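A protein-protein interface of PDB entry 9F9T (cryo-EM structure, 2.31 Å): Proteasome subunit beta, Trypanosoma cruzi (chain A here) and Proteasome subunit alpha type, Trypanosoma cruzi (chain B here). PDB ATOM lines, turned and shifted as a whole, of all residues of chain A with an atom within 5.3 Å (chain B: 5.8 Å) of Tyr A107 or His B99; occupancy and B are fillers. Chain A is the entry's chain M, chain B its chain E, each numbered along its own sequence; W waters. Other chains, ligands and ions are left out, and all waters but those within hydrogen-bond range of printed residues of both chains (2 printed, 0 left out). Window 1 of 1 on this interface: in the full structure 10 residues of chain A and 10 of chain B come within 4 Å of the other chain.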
ATOM      1  N   TYR A 102      -3.986  -5.196  19.142  1.00  0.00           N
ATOM      2  CA  TYR A 102      -5.261  -5.896  19.313  1.00  0.00           C
ATOM      3  C   TYR A 102      -6.442  -4.935  19.392  1.00  0.00           C
ATOM      4  O   TYR A 102      -7.507  -5.256  18.934  1.00  0.00           O
ATOM      5  CB  TYR A 102      -5.102  -6.818  20.534  1.00  0.00           C
ATOM      6  CG  TYR A 102      -4.081  -7.929  20.210  1.00  0.00           C
ATOM      7  CD1 TYR A 102      -4.241  -8.699  19.085  1.00  0.00           C
ATOM      8  CD2 TYR A 102      -2.935  -8.160  20.958  1.00  0.00           C
ATOM      9  CE1 TYR A 102      -3.354  -9.710  18.760  1.00  0.00           C
ATOM     10  CE2 TYR A 102      -1.990  -9.137  20.622  1.00  0.00           C
ATOM     11  CZ  TYR A 102      -2.218  -9.952  19.520  1.00  0.00           C
ATOM     12  OH  TYR A 102      -1.415 -10.974  19.066  1.00  0.00           O
ATOM     13  N   ARG A 103      -6.300  -3.750  19.961  1.00  0.00           N
ATOM     14  CA  ARG A 103      -7.329  -2.767  19.770  1.00  0.00           C
ATOM     15  C   ARG A 103      -7.536  -2.491  18.291  1.00  0.00           C
ATOM     16  O   ARG A 103      -8.666  -2.249  17.875  1.00  0.00           O
ATOM     17  CB  ARG A 103      -7.019  -1.465  20.446  1.00  0.00           C
ATOM     18  CG  ARG A 103      -7.020  -1.558  21.963  1.00  0.00           C
ATOM     19  CD  ARG A 103      -8.358  -1.823  22.610  1.00  0.00           C
ATOM     20  NE  ARG A 103      -9.242  -0.753  22.206  1.00  0.00           N
ATOM     21  CZ  ARG A 103      -9.582   0.242  23.014  1.00  0.00           C
ATOM     22  NH1 ARG A 103     -10.621   0.988  22.709  1.00  0.00           N
ATOM     23  NH2 ARG A 103      -8.933   0.423  24.160  1.00  0.00           N
ATOM     24  N   ILE A 104      -6.484  -2.587  17.488  1.00  0.00           N
ATOM     25  CA  ILE A 104      -6.610  -2.269  16.080  1.00  0.00           C
ATOM     26  C   ILE A 104      -7.245  -3.415  15.366  1.00  0.00           C
ATOM     27  O   ILE A 104      -8.077  -3.150  14.524  1.00  0.00           O
ATOM     28  CB  ILE A 104      -5.308  -1.840  15.400  1.00  0.00           C
ATOM     29  CG1 ILE A 104      -4.870  -0.517  15.958  1.00  0.00           C
ATOM     30  CG2 ILE A 104      -5.367  -1.823  13.910  1.00  0.00           C
ATOM     31  CD1 ILE A 104      -3.604  -0.084  15.352  1.00  0.00           C
ATOM     32  N   GLN A 105      -6.956  -4.627  15.780  1.00  0.00           N
ATOM     33  CA  GLN A 105      -7.658  -5.766  15.183  1.00  0.00           C
ATOM     34  C   GLN A 105      -9.155  -5.749  15.546  1.00  0.00           C
ATOM     35  O   GLN A 105     -10.017  -5.981  14.708  1.00  0.00           O
ATOM     36  CB  GLN A 105      -6.905  -7.054  15.532  1.00  0.00           C
ATOM     37  CG  GLN A 105      -7.124  -8.138  14.487  1.00  0.00           C
ATOM     38  CD  GLN A 105      -6.086  -9.253  14.400  1.00  0.00           C
ATOM     39  OE1 GLN A 105      -5.911  -9.851  13.330  1.00  0.00           O
ATOM     40  NE2 GLN A 105      -5.470  -9.619  15.521  1.00  0.00           N
ATOM     41  N   TRP A 106      -9.467  -5.321  16.759  1.00  0.00           N
ATOM     42  CA  TRP A 106     -10.847  -5.233  17.148  1.00  0.00           C
ATOM     43  C   TRP A 106     -11.560  -4.137  16.369  1.00  0.00           C
ATOM     44  O   TRP A 106     -12.712  -4.303  16.085  1.00  0.00           O
ATOM     45  CB  TRP A 106     -11.058  -5.029  18.658  1.00  0.00           C
ATOM     46  CG  TRP A 106     -11.021  -6.300  19.437  1.00  0.00           C
ATOM     47  CD1 TRP A 106     -10.064  -6.639  20.338  1.00  0.00           C
ATOM     48  CD2 TRP A 106     -11.902  -7.431  19.311  1.00  0.00           C
ATOM     49  NE1 TRP A 106     -10.306  -7.897  20.811  1.00  0.00           N
ATOM     50  CE2 TRP A 106     -11.425  -8.411  20.210  1.00  0.00           C
ATOM     51  CE3 TRP A 106     -13.042  -7.702  18.553  1.00  0.00           C
ATOM     52  CZ2 TRP A 106     -12.026  -9.655  20.360  1.00  0.00           C
ATOM     53  CZ3 TRP A 106     -13.641  -8.934  18.690  1.00  0.00           C
ATOM     54  CH2 TRP A 106     -13.110  -9.907  19.553  1.00  0.00           C
ATOM     55  N   TYR A 107     -10.936  -3.008  16.142  1.00  0.00           N
ATOM     56  CA  TYR A 107     -11.593  -1.992  15.358  1.00  0.00           C
ATOM     57  C   TYR A 107     -12.031  -2.567  14.005  1.00  0.00           C
ATOM     58  O   TYR A 107     -13.140  -2.277  13.576  1.00  0.00           O
ATOM     59  CB  TYR A 107     -10.574  -0.914  15.064  1.00  0.00           C
ATOM     60  CG  TYR A 107     -11.117   0.264  14.299  1.00  0.00           C
ATOM     61  CD1 TYR A 107     -10.978   0.351  12.938  1.00  0.00           C
ATOM     62  CD2 TYR A 107     -11.559   1.398  14.981  1.00  0.00           C
ATOM     63  CE1 TYR A 107     -11.379   1.484  12.248  1.00  0.00           C
ATOM     64  CE2 TYR A 107     -11.959   2.537  14.315  1.00  0.00           C
ATOM     65  CZ  TYR A 107     -11.900   2.557  12.932  1.00  0.00           C
ATOM     66  OH  TYR A 107     -12.254   3.681  12.250  1.00  0.00           O
ATOM     67  N   GLN A 108     -11.156  -3.385  13.373  1.00  0.00           N
ATOM     68  CA  GLN A 108     -11.394  -3.833  12.046  1.00  0.00           C
ATOM     69  C   GLN A 108     -12.611  -4.751  12.026  1.00  0.00           C
ATOM     70  O   GLN A 108     -13.462  -4.752  11.107  1.00  0.00           O
ATOM     71  CB  GLN A 108     -10.248  -4.641  11.504  1.00  0.00           C
ATOM     72  CG  GLN A 108      -9.189  -3.847  10.801  1.00  0.00           C
ATOM     73  CD  GLN A 108      -8.193  -4.790  10.147  1.00  0.00           C
ATOM     74  OE1 GLN A 108      -7.436  -5.479  10.817  1.00  0.00           O
ATOM     75  NE2 GLN A 108      -8.202  -4.868   8.829  1.00  0.00           N
ATOM     76  N   TYR A 109     -12.667  -5.626  13.030  1.00  0.00           N
ATOM     77  CA  TYR A 109     -13.752  -6.578  13.123  1.00  0.00           C
ATOM     78  C   TYR A 109     -15.037  -5.830  13.369  1.00  0.00           C
ATOM     79  O   TYR A 109     -16.014  -6.243  12.803  1.00  0.00           O
ATOM     80  CB  TYR A 109     -13.554  -7.598  14.237  1.00  0.00           C
ATOM     81  CG  TYR A 109     -12.406  -8.574  14.037  1.00  0.00           C
ATOM     82  CD1 TYR A 109     -12.098  -9.092  12.816  1.00  0.00           C
ATOM     83  CD2 TYR A 109     -11.672  -9.040  15.115  1.00  0.00           C
ATOM     84  CE1 TYR A 109     -11.174 -10.130  12.691  1.00  0.00           C
ATOM     85  CE2 TYR A 109     -10.665  -9.988  14.991  1.00  0.00           C
ATOM     86  CZ  TYR A 109     -10.447 -10.565  13.772  1.00  0.00           C
ATOM     87  OH  TYR A 109      -9.498 -11.533  13.643  1.00  0.00           O
ATOM     88  N   ASN A 110     -15.025  -4.728  14.124  1.00  0.00           N
ATOM     89  CA  ASN A 110     -16.248  -3.997  14.442  1.00  0.00           C
ATOM     90  C   ASN A 110     -16.598  -2.914  13.401  1.00  0.00           C
ATOM     91  O   ASN A 110     -17.527  -2.135  13.600  1.00  0.00           O
ATOM     92  CB  ASN A 110     -16.148  -3.223  15.772  1.00  0.00           C
ATOM     93  CG  ASN A 110     -15.925  -4.084  17.000  1.00  0.00           C
ATOM     94  OD1 ASN A 110     -16.396  -5.216  17.080  1.00  0.00           O
ATOM     95  ND2 ASN A 110     -15.218  -3.559  17.981  1.00  0.00           N
ATOM     96  N   ASN A 111     -15.765  -2.775  12.361  1.00  0.00           N
ATOM     97  CA  ASN A 111     -15.857  -1.665  11.430  1.00  0.00           C
ATOM     98  C   ASN A 111     -15.783  -2.167  10.003  1.00  0.00           C
ATOM     99  O   ASN A 111     -15.306  -1.466   9.124  1.00  0.00           O
ATOM    100  CB  ASN A 111     -14.764  -0.619  11.558  1.00  0.00           C
ATOM    101  CG  ASN A 111     -15.047   0.353  12.686  1.00  0.00           C
ATOM    102  OD1 ASN A 111     -15.507   1.492  12.502  1.00  0.00           O
ATOM    103  ND2 ASN A 111     -14.786  -0.092  13.895  1.00  0.00           N
ATOM    104  N   GLY A 112     -16.241  -3.370   9.756  1.00  0.00           N
ATOM    105  CA  GLY A 112     -16.396  -3.732   8.373  1.00  0.00           C
ATOM    106  C   GLY A 112     -15.068  -3.961   7.674  1.00  0.00           C
ATOM    107  O   GLY A 112     -15.017  -3.942   6.438  1.00  0.00           O
ATOM    108  N   LYS A 114     -12.271  -2.246   7.905  1.00  0.00           N
ATOM    109  CA  LYS A 114     -11.464  -1.061   7.657  1.00  0.00           C
ATOM    110  C   LYS A 114     -10.436  -0.865   8.755  1.00  0.00           C
ATOM    111  O   LYS A 114     -10.666  -1.209   9.900  1.00  0.00           O
ATOM    112  CB  LYS A 114     -12.318   0.209   7.639  1.00  0.00           C
ATOM    113  CG  LYS A 114     -12.832   0.642   6.270  1.00  0.00           C
ATOM    114  CD  LYS A 114     -14.148   0.029   5.935  1.00  0.00           C
ATOM    115  CE  LYS A 114     -14.413   0.015   4.441  1.00  0.00           C
ATOM    116  NZ  LYS A 114     -15.748  -0.559   4.126  1.00  0.00           N
ATOM    117  N   LEU A 115      -9.364  -0.156   8.425  1.00  0.00           N
ATOM    118  CA  LEU A 115      -8.336   0.214   9.374  1.00  0.00           C
ATOM    119  C   LEU A 115      -8.540   1.616   9.851  1.00  0.00           C
ATOM    120  O   LEU A 115      -8.910   2.470   9.091  1.00  0.00           O
ATOM    121  CB  LEU A 115      -7.000   0.107   8.662  1.00  0.00           C
ATOM    122  CG  LEU A 115      -6.587  -1.350   8.438  1.00  0.00           C
ATOM    123  CD1 LEU A 115      -5.429  -1.439   7.462  1.00  0.00           C
ATOM    124  CD2 LEU A 115      -6.235  -2.025   9.762  1.00  0.00           C
ATOM    125  N   PRO A 116      -8.230   1.917  11.104  1.00  0.00           N
ATOM    126  CA  PRO A 116      -8.325   3.271  11.576  1.00  0.00           C
ATOM    127  C   PRO A 116      -7.175   4.044  10.929  1.00  0.00           C
ATOM    128  O   PRO A 116      -6.092   3.487  10.701  1.00  0.00           O
ATOM    129  CB  PRO A 116      -8.191   3.069  13.101  1.00  0.00           C
ATOM    130  CG  PRO A 116      -7.249   1.872  13.262  1.00  0.00           C
ATOM    131  CD  PRO A 116      -7.618   1.025  12.082  1.00  0.00           C
ATOM    132  N   VAL B  94     -24.800   6.230  23.501  1.00  0.00           N
ATOM    133  CA  VAL B  94     -23.600   6.142  24.328  1.00  0.00           C
ATOM    134  C   VAL B  94     -22.456   5.533  23.508  1.00  0.00           C
ATOM    135  O   VAL B  94     -21.338   6.057  23.520  1.00  0.00           O
ATOM    136  CB  VAL B  94     -23.863   5.379  25.642  1.00  0.00           C
ATOM    137  CG1 VAL B  94     -22.584   4.912  26.304  1.00  0.00           C
ATOM    138  CG2 VAL B  94     -24.640   6.255  26.586  1.00  0.00           C
ATOM    139  N   GLU B  95     -22.720   4.481  22.757  1.00  0.00           N
ATOM    140  CA  GLU B  95     -21.672   3.928  21.911  1.00  0.00           C
ATOM    141  C   GLU B  95     -21.143   4.933  20.869  1.00  0.00           C
ATOM    142  O   GLU B  95     -19.976   4.901  20.470  1.00  0.00           O
ATOM    143  CB  GLU B  95     -22.181   2.681  21.205  1.00  0.00           C
ATOM    144  CG  GLU B  95     -22.355   1.511  22.174  1.00  0.00           C
ATOM    145  CD  GLU B  95     -21.081   1.067  22.910  1.00  0.00           C
ATOM    146  OE1 GLU B  95     -20.042   0.853  22.215  1.00  0.00           O
ATOM    147  OE2 GLU B  95     -21.111   0.928  24.184  1.00  0.00           O
ATOM    148  N   ALA B  96     -21.990   5.844  20.407  1.00  0.00           N
ATOM    149  CA  ALA B  96     -21.570   6.644  19.309  1.00  0.00           C
ATOM    150  C   ALA B  96     -20.619   7.698  19.836  1.00  0.00           C
ATOM    151  O   ALA B  96     -19.834   8.265  19.072  1.00  0.00           O
ATOM    152  CB  ALA B  96     -22.757   7.242  18.598  1.00  0.00           C
ATOM    153  N   GLN B  97     -20.820   8.030  21.098  1.00  0.00           N
ATOM    154  CA  GLN B  97     -20.036   9.037  21.755  1.00  0.00           C
ATOM    155  C   GLN B  97     -18.798   8.357  22.331  1.00  0.00           C
ATOM    156  O   GLN B  97     -17.832   9.066  22.568  1.00  0.00           O
ATOM    157  CB  GLN B  97     -20.716   9.773  22.948  1.00  0.00           C
ATOM    158  CG  GLN B  97     -21.667  10.936  22.674  1.00  0.00           C
ATOM    159  CD  GLN B  97     -21.286  11.833  21.534  1.00  0.00           C
ATOM    160  OE1 GLN B  97     -20.369  12.666  21.599  1.00  0.00           O
ATOM    161  NE2 GLN B  97     -21.976  11.625  20.424  1.00  0.00           N
ATOM    162  N   ASN B  98     -18.824   7.087  22.682  1.00  0.00           N
ATOM    163  CA  ASN B  98     -17.578   6.453  23.100  1.00  0.00           C
ATOM    164  C   ASN B  98     -16.606   6.355  21.929  1.00  0.00           C
ATOM    165  O   ASN B  98     -15.482   6.818  22.020  1.00  0.00           O
ATOM    166  CB  ASN B  98     -17.732   5.051  23.634  1.00  0.00           C
ATOM    167  CG  ASN B  98     -18.276   5.061  25.037  1.00  0.00           C
ATOM    168  OD1 ASN B  98     -18.014   5.979  25.803  1.00  0.00           O
ATOM    169  ND2 ASN B  98     -19.078   4.070  25.372  1.00  0.00           N
ATOM    170  N   HIS B  99     -17.089   5.928  20.786  1.00  0.00           N
ATOM    171  CA  HIS B  99     -16.286   5.985  19.609  1.00  0.00           C
ATOM    172  C   HIS B  99     -15.611   7.334  19.417  1.00  0.00           C
ATOM    173  O   HIS B  99     -14.439   7.375  19.107  1.00  0.00           O
ATOM    174  CB  HIS B  99     -17.118   5.651  18.392  1.00  0.00           C
ATOM    175  CG  HIS B  99     -16.299   5.183  17.273  1.00  0.00           C
ATOM    176  ND1 HIS B  99     -15.866   3.869  17.227  1.00  0.00           N
ATOM    177  CD2 HIS B  99     -15.819   5.819  16.161  1.00  0.00           C
ATOM    178  CE1 HIS B  99     -15.136   3.721  16.103  1.00  0.00           C
ATOM    179  NE2 HIS B  99     -15.133   4.891  15.423  1.00  0.00           N
ATOM    180  N   ARG B 100     -16.364   8.441  19.427  1.00  0.00           N
ATOM    181  CA  ARG B 100     -15.733   9.712  19.169  1.00  0.00           C
ATOM    182  C   ARG B 100     -14.723  10.076  20.239  1.00  0.00           C
ATOM    183  O   ARG B 100     -13.765  10.798  19.983  1.00  0.00           O
ATOM    184  CB  ARG B 100     -16.687  10.877  19.279  1.00  0.00           C
ATOM    185  CG  ARG B 100     -17.538  11.012  18.047  1.00  0.00           C
ATOM    186  CD  ARG B 100     -18.239  12.346  18.183  1.00  0.00           C
ATOM    187  NE  ARG B 100     -19.151  12.394  17.055  1.00  0.00           N
ATOM    188  CZ  ARG B 100     -18.966  13.144  15.982  1.00  0.00           C
ATOM    189  NH1 ARG B 100     -17.963  14.007  15.966  1.00  0.00           N
ATOM    190  NH2 ARG B 100     -19.801  13.031  14.961  1.00  0.00           N
ATOM    191  N   PHE B 101     -15.033   9.695  21.468  1.00  0.00           N
ATOM    192  CA  PHE B 101     -14.091   9.879  22.542  1.00  0.00           C
ATOM    193  C   PHE B 101     -12.826   9.149  22.178  1.00  0.00           C
ATOM    194  O   PHE B 101     -11.849   9.825  22.036  1.00  0.00           O
ATOM    195  CB  PHE B 101     -14.676   9.428  23.859  1.00  0.00           C
ATOM    196  CG  PHE B 101     -13.744   9.620  25.012  1.00  0.00           C
ATOM    197  CD1 PHE B 101     -13.672  10.823  25.645  1.00  0.00           C
ATOM    198  CD2 PHE B 101     -12.871   8.622  25.385  1.00  0.00           C
ATOM    199  CE1 PHE B 101     -12.783  11.010  26.681  1.00  0.00           C
ATOM    200  CE2 PHE B 101     -11.959   8.809  26.409  1.00  0.00           C
ATOM    201  CZ  PHE B 101     -11.920   9.991  27.052  1.00  0.00           C
ATOM    202  N   THR B 102     -12.872   7.845  21.891  1.00  0.00           N
ATOM    203  CA  THR B 102     -11.679   7.019  21.782  1.00  0.00           C
ATOM    204  C   THR B 102     -10.944   7.306  20.485  1.00  0.00           C
ATOM    205  O   THR B 102      -9.743   7.385  20.486  1.00  0.00           O
ATOM    206  CB  THR B 102     -11.964   5.523  21.905  1.00  0.00           C
ATOM    207  OG1 THR B 102     -12.409   5.120  23.203  1.00  0.00           O
ATOM    208  CG2 THR B 102     -10.757   4.643  21.704  1.00  0.00           C
ATOM    209  N   TYR B 103     -11.585   7.511  19.363  1.00  0.00           N
ATOM    210  CA  TYR B 103     -10.840   7.638  18.139  1.00  0.00           C
ATOM    211  C   TYR B 103     -11.145   8.880  17.322  1.00  0.00           C
ATOM    212  O   TYR B 103     -11.027   8.809  16.097  1.00  0.00           O
ATOM    213  CB  TYR B 103     -11.388   6.557  17.233  1.00  0.00           C
ATOM    214  CG  TYR B 103     -11.270   5.155  17.757  1.00  0.00           C
ATOM    215  CD1 TYR B 103     -10.150   4.382  17.548  1.00  0.00           C
ATOM    216  CD2 TYR B 103     -12.368   4.550  18.321  1.00  0.00           C
ATOM    217  CE1 TYR B 103     -10.066   3.091  18.025  1.00  0.00           C
ATOM    218  CE2 TYR B 103     -12.322   3.248  18.770  1.00  0.00           C
ATOM    219  CZ  TYR B 103     -11.168   2.510  18.630  1.00  0.00           C
ATOM    220  OH  TYR B 103     -11.245   1.207  19.094  1.00  0.00           O
ATOM    221  N   ASP B 104     -11.833   9.858  17.912  1.00  0.00           N
ATOM    222  CA  ASP B 104     -11.954  11.218  17.395  1.00  0.00           C
ATOM    223  C   ASP B 104     -12.583  11.318  16.023  1.00  0.00           C
ATOM    224  O   ASP B 104     -12.232  12.199  15.249  1.00  0.00           O
ATOM    225  CB  ASP B 104     -10.586  11.875  17.248  1.00  0.00           C
ATOM    226  CG  ASP B 104     -10.715  13.392  17.187  1.00  0.00           C
ATOM    227  OD1 ASP B 104     -11.726  13.919  17.740  1.00  0.00           O
ATOM    228  OD2 ASP B 104      -9.830  14.054  16.566  1.00  0.00           O
ATOM    229  N   GLU B 105     -13.525  10.423  15.737  1.00  0.00           N
ATOM    230  CA  GLU B 105     -14.213  10.461  14.466  1.00  0.00           C
ATOM    231  C   GLU B 105     -15.600   9.842  14.620  1.00  0.00           C
ATOM    232  O   GLU B 105     -15.855   9.069  15.530  1.00  0.00           O
ATOM    233  CB  GLU B 105     -13.419   9.644  13.433  1.00  0.00           C
ATOM    234  CG  GLU B 105     -13.586   8.143  13.633  1.00  0.00           C
ATOM    235  CD  GLU B 105     -12.616   7.106  13.098  1.00  0.00           C
ATOM    236  OE1 GLU B 105     -11.581   7.485  12.522  1.00  0.00           O
ATOM    237  OE2 GLU B 105     -12.929   5.861  13.271  1.00  0.00           O
ATOM    238  N   PRO B 106     -16.521  10.028  13.650  1.00  0.00           N
ATOM    239  CA  PRO B 106     -17.863   9.471  13.777  1.00  0.00           C
ATOM    240  C   PRO B 106     -17.915   7.971  13.620  1.00  0.00           C
ATOM    241  O   PRO B 106     -17.289   7.403  12.742  1.00  0.00           O
ATOM    242  CB  PRO B 106     -18.656  10.111  12.650  1.00  0.00           C
ATOM    243  CG  PRO B 106     -17.835  11.317  12.286  1.00  0.00           C
ATOM    244  CD  PRO B 106     -16.391  10.854  12.437  1.00  0.00           C
ATOM    245  N   MET B 107     -18.795   7.376  14.393  1.00  0.00           N
ATOM    246  CA  MET B 107     -19.084   5.970  14.289  1.00  0.00           C
ATOM    247  C   MET B 107     -19.693   5.728  12.914  1.00  0.00           C
ATOM    248  O   MET B 107     -20.464   6.555  12.407  1.00  0.00           O
ATOM    249  CB  MET B 107     -20.026   5.599  15.446  1.00  0.00           C
ATOM    250  CG  MET B 107     -20.317   4.153  15.560  1.00  0.00           C
ATOM    251  SD  MET B 107     -20.873   3.675  17.204  1.00  0.00           S
ATOM    252  CE  MET B 107     -20.125   2.053  17.333  1.00  0.00           C
ATOM    253  N   ARG B 108     -19.267   4.639  12.283  1.00  0.00           N
ATOM    254  CA  ARG B 108     -19.928   4.153  11.089  1.00  0.00           C
ATOM    255  C   ARG B 108     -21.325   3.708  11.517  1.00  0.00           C
ATOM    256  O   ARG B 108     -21.559   3.331  12.663  1.00  0.00           O
ATOM    257  CB  ARG B 108     -19.155   3.001  10.413  1.00  0.00           C
ATOM    258  CG  ARG B 108     -17.822   3.409   9.785  1.00  0.00           C
ATOM    259  CD  ARG B 108     -16.899   2.266   9.319  1.00  0.00           C
ATOM    260  NE  ARG B 108     -15.698   2.796   8.625  1.00  0.00           N
ATOM    261  CZ  ARG B 108     -14.638   3.427   9.188  1.00  0.00           C
ATOM    262  NH1 ARG B 108     -14.354   3.330  10.472  1.00  0.00           N
ATOM    263  NH2 ARG B 108     -13.793   4.113   8.441  1.00  0.00           N
HETATM  264  O   HOH W   1     -13.252  -0.873  18.204  1.00  0.00           O
HETATM  265  O   HOH W   2     -10.982   3.867   8.785  1.00  0.00           O
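The backbone carbonyl oxygen of Tyr A107 sits at hydrogen-bond distance from the side-chain amide nitrogen of Asn A111 (2.8 Å). OE2 of Glu B105 is in hydrogen-bond range of NE2 of His B99 (3.2 Å).
Tyr A102 touches none of the printed residues of chain B. Tyr A107 touches just these residues of chain B: His B99 (3.8 Å), Tyr B103 (3.8 Å), Glu B105 (2.5 Å) and Arg B108 (2.8 Å). Gln B97 touches none of the printed residues of chain A. Printed residues of chain A within 4 Å of Tyr B103: Arg A103 and Tyr A107. Of the printed residues of chain A, Arg B108 touches Tyr A107 (2.8 Å) and Asn A111 (3.0 Å). The nearest printed residue of chain B that does not touch Tyr A107 is Pro B106 (6.3 Å). The nearest residue of chain A that does not touch His B99 is Asn A111 (4.3 Å). The nearest printed residue of chain A that does not touch Glu B105 is Asn A111 (5.1 Å).
Arg A103 touches Thr B102 (NH1 to CG2, 3.8 Å). Arg A103 touches Tyr B103 (NH1 to OH, 3.7 Å). His B99 touches Tyr A107. CD2 of Tyr A107 touches CE1 of Tyr B103, 3.8 Å away.
Printed residues of chain A that touch a printed residue of chain B: Arg A103, Tyr A107 and Asn A111. Hydrophobic or aromatic side chains of chain A that line the printed part of chain B: Tyr A107. Of the 15 printed residues of chain B, 5 touch a printed residue of chain A. Hydrophobic or aromatic side chains of chain B that line the printed part of chain A: His B99 and Tyr B103. Among the printed residues, 7 pairs touch across the chains.
The side-chain hydroxyl (OH) of Tyr A107 is in hydrogen-bond range of the side-chain carboxylate (OE2) of Glu B105. OH of Tyr A107 lies within hydrogen-bond range of NH1 of Arg B108 (2.8 Å). The guanidinium group (NH1) of Arg B108 lies within hydrogen-bond range of the side-chain amide oxygen (OD1) of Asn A111, 3.0 Å away.
Water W2 bridges O of Leu A115 (2.5 Å) and NH2 of Arg B108 (2.8 Å). Water W1 bridges OH of Tyr B103 (3.0 Å) and ND2 of Asn A110 (3.3 Å).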
